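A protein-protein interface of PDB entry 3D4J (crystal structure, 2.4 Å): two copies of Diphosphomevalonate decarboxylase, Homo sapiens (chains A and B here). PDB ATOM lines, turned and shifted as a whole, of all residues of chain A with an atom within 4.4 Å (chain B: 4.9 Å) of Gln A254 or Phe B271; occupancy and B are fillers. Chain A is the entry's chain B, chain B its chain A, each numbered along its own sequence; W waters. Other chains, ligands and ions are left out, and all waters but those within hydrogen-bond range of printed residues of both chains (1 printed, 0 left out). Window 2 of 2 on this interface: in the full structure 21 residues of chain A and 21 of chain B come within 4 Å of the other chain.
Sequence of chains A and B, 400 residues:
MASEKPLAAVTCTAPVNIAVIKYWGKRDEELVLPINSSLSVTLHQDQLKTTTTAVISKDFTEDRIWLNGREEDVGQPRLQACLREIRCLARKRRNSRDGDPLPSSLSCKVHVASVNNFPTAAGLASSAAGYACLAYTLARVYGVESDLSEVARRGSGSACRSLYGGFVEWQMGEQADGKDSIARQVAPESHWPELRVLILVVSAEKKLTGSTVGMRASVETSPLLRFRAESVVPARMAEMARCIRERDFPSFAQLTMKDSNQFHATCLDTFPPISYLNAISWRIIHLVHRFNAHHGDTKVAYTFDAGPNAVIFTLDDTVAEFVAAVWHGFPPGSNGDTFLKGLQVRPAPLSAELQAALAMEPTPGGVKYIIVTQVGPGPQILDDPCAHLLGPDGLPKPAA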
ATOM      1  N   PRO A 250       9.984  -5.964   3.475  1.00  0.00           N
ATOM      2  CA  PRO A 250       9.256  -7.230   3.340  1.00  0.00           C
ATOM      3  C   PRO A 250       8.951  -7.659   1.901  1.00  0.00           C
ATOM      4  O   PRO A 250       8.985  -8.846   1.605  1.00  0.00           O
ATOM      5  CB  PRO A 250       7.994  -7.009   4.186  1.00  0.00           C
ATOM      6  CG  PRO A 250       7.879  -5.526   4.299  1.00  0.00           C
ATOM      7  CD  PRO A 250       9.300  -5.060   4.410  1.00  0.00           C
ATOM      8  N   SER A 251       8.660  -6.707   1.015  1.00  0.00           N
ATOM      9  CA  SER A 251       8.371  -7.052  -0.375  1.00  0.00           C
ATOM     10  C   SER A 251       9.683  -7.342  -1.080  1.00  0.00           C
ATOM     11  O   SER A 251       9.785  -8.246  -1.912  1.00  0.00           O
ATOM     12  CB  SER A 251       7.637  -5.905  -1.092  1.00  0.00           C
ATOM     13  OG  SER A 251       6.284  -5.807  -0.660  1.00  0.00           O
ATOM     14  N   PHE A 252      10.693  -6.552  -0.743  1.00  0.00           N
ATOM     15  CA  PHE A 252      12.014  -6.719  -1.318  1.00  0.00           C
ATOM     16  C   PHE A 252      12.555  -8.092  -0.937  1.00  0.00           C
ATOM     17  O   PHE A 252      13.224  -8.756  -1.738  1.00  0.00           O
ATOM     18  CB  PHE A 252      12.938  -5.635  -0.774  1.00  0.00           C
ATOM     19  CG  PHE A 252      14.394  -5.972  -0.870  1.00  0.00           C
ATOM     20  CD1 PHE A 252      15.129  -5.613  -1.989  1.00  0.00           C
ATOM     21  CD2 PHE A 252      15.032  -6.658   0.168  1.00  0.00           C
ATOM     22  CE1 PHE A 252      16.481  -5.926  -2.079  1.00  0.00           C
ATOM     23  CE2 PHE A 252      16.382  -6.977   0.088  1.00  0.00           C
ATOM     24  CZ  PHE A 252      17.110  -6.611  -1.034  1.00  0.00           C
ATOM     25  N   ALA A 253      12.249  -8.508   0.291  1.00  0.00           N
ATOM     26  CA  ALA A 253      12.720  -9.780   0.824  1.00  0.00           C
ATOM     27  C   ALA A 253      12.052 -10.972   0.179  1.00  0.00           C
ATOM     28  O   ALA A 253      12.722 -11.930  -0.214  1.00  0.00           O
ATOM     29  CB  ALA A 253      12.507  -9.826   2.331  1.00  0.00           C
ATOM     30  N   GLN A 254      10.731 -10.925   0.080  1.00  0.00           N
ATOM     31  CA  GLN A 254       9.993 -12.030  -0.521  1.00  0.00           C
ATOM     32  C   GLN A 254      10.377 -12.244  -1.978  1.00  0.00           C
ATOM     33  O   GLN A 254      10.619 -13.376  -2.401  1.00  0.00           O
ATOM     34  CB  GLN A 254       8.488 -11.799  -0.410  1.00  0.00           C
ATOM     35  CG  GLN A 254       8.005 -11.669   1.012  1.00  0.00           C
ATOM     36  CD  GLN A 254       6.508 -11.855   1.148  1.00  0.00           C
ATOM     37  OE1 GLN A 254       5.915 -11.433   2.139  1.00  0.00           O
ATOM     38  NE2 GLN A 254       5.889 -12.503   0.161  1.00  0.00           N
ATOM     39  N   LEU A 255      10.441 -11.157  -2.738  1.00  0.00           N
ATOM     40  CA  LEU A 255      10.807 -11.234  -4.145  1.00  0.00           C
ATOM     41  C   LEU A 255      12.213 -11.829  -4.263  1.00  0.00           C
ATOM     42  O   LEU A 255      12.453 -12.712  -5.094  1.00  0.00           O
ATOM     43  CB  LEU A 255      10.785  -9.839  -4.784  1.00  0.00           C
ATOM     44  CG  LEU A 255      10.173  -9.683  -6.182  1.00  0.00           C
ATOM     45  CD1 LEU A 255      10.745  -8.421  -6.834  1.00  0.00           C
ATOM     46  CD2 LEU A 255      10.473 -10.918  -7.044  1.00  0.00           C
ATOM     47  N   THR A 256      13.140 -11.343  -3.436  1.00  0.00           N
ATOM     48  CA  THR A 256      14.509 -11.850  -3.465  1.00  0.00           C
ATOM     49  C   THR A 256      14.510 -13.361  -3.241  1.00  0.00           C
ATOM     50  O   THR A 256      15.169 -14.093  -3.966  1.00  0.00           O
ATOM     51  CB  THR A 256      15.410 -11.184  -2.383  1.00  0.00           C
ATOM     52  OG1 THR A 256      15.533  -9.775  -2.641  1.00  0.00           O
ATOM     53  CG2 THR A 256      16.796 -11.816  -2.391  1.00  0.00           C
ATOM     54  N   MET A 257      13.760 -13.832  -2.248  1.00  0.00           N
ATOM     55  CA  MET A 257      13.697 -15.265  -1.966  1.00  0.00           C
ATOM     56  C   MET A 257      13.026 -16.051  -3.080  1.00  0.00           C
ATOM     57  O   MET A 257      13.460 -17.143  -3.425  1.00  0.00           O
ATOM     58  CB  MET A 257      12.947 -15.535  -0.659  1.00  0.00           C
ATOM     59  CG  MET A 257      13.713 -15.142   0.612  1.00  0.00           C
ATOM     60  SD  MET A 257      12.794 -15.547   2.114  1.00  0.00           S
ATOM     61  CE  MET A 257      11.624 -14.165   2.188  1.00  0.00           C
ATOM     62  N   LYS A 258      11.943 -15.511  -3.622  1.00  0.00           N
ATOM     63  CA  LYS A 258      11.244 -16.198  -4.690  1.00  0.00           C
ATOM     64  C   LYS A 258      12.145 -16.320  -5.915  1.00  0.00           C
ATOM     65  O   LYS A 258      12.142 -17.343  -6.589  1.00  0.00           O
ATOM     66  CB  LYS A 258       9.956 -15.450  -5.045  1.00  0.00           C
ATOM     67  CG  LYS A 258       8.832 -15.655  -4.031  1.00  0.00           C
ATOM     68  CD  LYS A 258       7.704 -14.642  -4.205  1.00  0.00           C
ATOM     69  CE  LYS A 258       6.560 -14.923  -3.232  1.00  0.00           C
ATOM     70  NZ  LYS A 258       5.653 -13.756  -3.040  1.00  0.00           N
ATOM     71  N   HIS A 289      12.367 -18.703   7.242  1.00  0.00           N
ATOM     72  CA  HIS A 289      10.923 -18.711   7.226  1.00  0.00           C
ATOM     73  C   HIS A 289      10.345 -18.840   8.619  1.00  0.00           C
ATOM     74  O   HIS A 289       9.310 -18.235   8.928  1.00  0.00           O
ATOM     75  CB  HIS A 289      10.416 -19.835   6.324  1.00  0.00           C
ATOM     76  CG  HIS A 289      10.630 -19.566   4.869  1.00  0.00           C
ATOM     77  ND1 HIS A 289      10.178 -18.419   4.257  1.00  0.00           N
ATOM     78  CD2 HIS A 289      11.295 -20.262   3.916  1.00  0.00           C
ATOM     79  CE1 HIS A 289      10.560 -18.413   2.992  1.00  0.00           C
ATOM     80  NE2 HIS A 289      11.240 -19.523   2.761  1.00  0.00           N
ATOM     81  N   THR A 298       7.983 -10.389   7.428  1.00  0.00           N
ATOM     82  CA  THR A 298       9.190 -10.767   6.716  1.00  0.00           C
ATOM     83  C   THR A 298      10.307  -9.816   7.140  1.00  0.00           C
ATOM     84  O   THR A 298      10.353  -8.660   6.700  1.00  0.00           O
ATOM     85  CB  THR A 298       8.998 -10.683   5.190  1.00  0.00           C
ATOM     86  OG1 THR A 298       7.761 -11.309   4.823  1.00  0.00           O
ATOM     87  CG2 THR A 298      10.138 -11.393   4.487  1.00  0.00           C
ATOM     88  N   THR B 221       1.387 -20.520  -5.439  1.00  0.00           N
ATOM     89  CA  THR B 221       2.580 -19.670  -5.539  1.00  0.00           C
ATOM     90  C   THR B 221       3.630 -19.897  -6.623  1.00  0.00           C
ATOM     91  O   THR B 221       4.508 -19.048  -6.799  1.00  0.00           O
ATOM     92  CB  THR B 221       3.365 -19.672  -4.186  1.00  0.00           C
ATOM     93  OG1 THR B 221       3.900 -20.984  -3.934  1.00  0.00           O
ATOM     94  CG2 THR B 221       2.449 -19.292  -3.023  1.00  0.00           C
ATOM     95  N   ASP B 269      10.234 -23.860  -6.633  1.00  0.00           N
ATOM     96  CA  ASP B 269       9.658 -22.581  -7.063  1.00  0.00           C
ATOM     97  C   ASP B 269       8.423 -22.213  -6.232  1.00  0.00           C
ATOM     98  O   ASP B 269       7.815 -21.171  -6.414  1.00  0.00           O
ATOM     99  CB  ASP B 269       9.272 -22.661  -8.543  1.00  0.00           C
ATOM    100  CG  ASP B 269       8.800 -21.328  -9.104  1.00  0.00           C
ATOM    101  OD1 ASP B 269       9.578 -20.352  -9.056  1.00  0.00           O
ATOM    102  OD2 ASP B 269       7.650 -21.262  -9.599  1.00  0.00           O
ATOM    103  N   THR B 270       8.034 -23.092  -5.328  1.00  0.00           N
ATOM    104  CA  THR B 270       6.898 -22.828  -4.470  1.00  0.00           C
ATOM    105  C   THR B 270       7.434 -21.899  -3.360  1.00  0.00           C
ATOM    106  O   THR B 270       8.649 -21.834  -3.138  1.00  0.00           O
ATOM    107  CB  THR B 270       6.351 -24.167  -3.895  1.00  0.00           C
ATOM    108  OG1 THR B 270       5.985 -25.023  -4.982  1.00  0.00           O
ATOM    109  CG2 THR B 270       5.125 -23.952  -3.010  1.00  0.00           C
ATOM    110  N   PHE B 271       6.542 -21.164  -2.693  1.00  0.00           N
ATOM    111  CA  PHE B 271       6.952 -20.243  -1.630  1.00  0.00           C
ATOM    112  C   PHE B 271       6.081 -20.416  -0.376  1.00  0.00           C
ATOM    113  O   PHE B 271       4.880 -20.176  -0.409  1.00  0.00           O
ATOM    114  CB  PHE B 271       6.871 -18.786  -2.121  1.00  0.00           C
ATOM    115  CG  PHE B 271       7.397 -17.775  -1.130  1.00  0.00           C
ATOM    116  CD1 PHE B 271       8.769 -17.576  -0.974  1.00  0.00           C
ATOM    117  CD2 PHE B 271       6.522 -17.075  -0.297  1.00  0.00           C
ATOM    118  CE1 PHE B 271       9.257 -16.704   0.000  1.00  0.00           C
ATOM    119  CE2 PHE B 271       7.002 -16.203   0.678  1.00  0.00           C
ATOM    120  CZ  PHE B 271       8.370 -16.018   0.826  1.00  0.00           C
ATOM    121  N   PRO B 272       6.680 -20.851   0.749  1.00  0.00           N
ATOM    122  CA  PRO B 272       8.097 -21.195   0.939  1.00  0.00           C
ATOM    123  C   PRO B 272       8.446 -22.369   0.027  1.00  0.00           C
ATOM    124  O   PRO B 272       7.558 -23.121  -0.376  1.00  0.00           O
ATOM    125  CB  PRO B 272       8.168 -21.585   2.421  1.00  0.00           C
ATOM    126  CG  PRO B 272       7.050 -20.813   3.026  1.00  0.00           C
ATOM    127  CD  PRO B 272       5.945 -20.957   2.019  1.00  0.00           C
ATOM    128  N   PRO B 273       9.741 -22.546  -0.301  1.00  0.00           N
ATOM    129  CA  PRO B 273      10.166 -23.649  -1.176  1.00  0.00           C
ATOM    130  C   PRO B 273      10.008 -25.017  -0.528  1.00  0.00           C
ATOM    131  O   PRO B 273      10.104 -25.145   0.686  1.00  0.00           O
ATOM    132  CB  PRO B 273      11.622 -23.309  -1.469  1.00  0.00           C
ATOM    133  CG  PRO B 273      12.060 -22.630  -0.213  1.00  0.00           C
ATOM    134  CD  PRO B 273      10.890 -21.716   0.090  1.00  0.00           C
HETATM  135  O   HOH W   1       9.819 -17.991  -7.797  1.00  0.00           O
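Hydrophobic or aromatic side chains of chain B within 4 Å of the printed part of chain A: Phe B271, Pro B272 and Pro B273. Of the 11 printed residues of chain A, 4 touch a printed residue of chain B. Hydrophobic or aromatic side chains of chain A within 4 Å of the printed part of chain B: Met A257 and His A289. Along chain A the printed residues that touch a printed residue of chain B span positions 254 to 289.
Of chain B, only Phe B271 comes within 4 Å of Gln A254. Phe B271 touches just these residues of chain A: Gln A254 (3.9 Å), Met A257 (3.9 Å), Lys A258 (3.6 Å) and His A289 (3.7 Å). Printed residues of chain B within 4 Å of His A289: Phe B271, Pro B272 and Pro B273. Of the printed residues of chain A, Pro B273 touches His A289. Of the printed residues of chain B, Lys A258 touches Phe B271. The nearest printed residue of chain A that does not touch Phe B271 is Ala A253 (5.9 Å).
No position is printed for both chains.
NE2 of Gln A254 touches CE2 of Phe B271, 3.9 Å away. Phe B271 touches Met A257 (CE1 to CB, 3.9 Å). CG of Lys A258 touches CD1 of Phe B271, 3.6 Å away. CE1 of His A289 touches CE1 of Phe B271, at 3.7 Å. His A289 touches Pro B272 (CD2 to CB, 3.7 Å). His A289 touches Pro B273.
Water W1 lies within hydrogen-bond range of OD1 of Asp B269 (2.7 Å) and O of Lys A258 (2.7 Å).
N of Phe B271 sits at hydrogen-bond distance from OG1 of Thr B221, at 2.9 Å. The side-chain amide oxygen of Gln A254 sits at hydrogen-bond distance from the side-chain hydroxyl of Thr A298, 3.3 Å away. NZ of Lys A258 sits close to NE2 of Gln A254.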
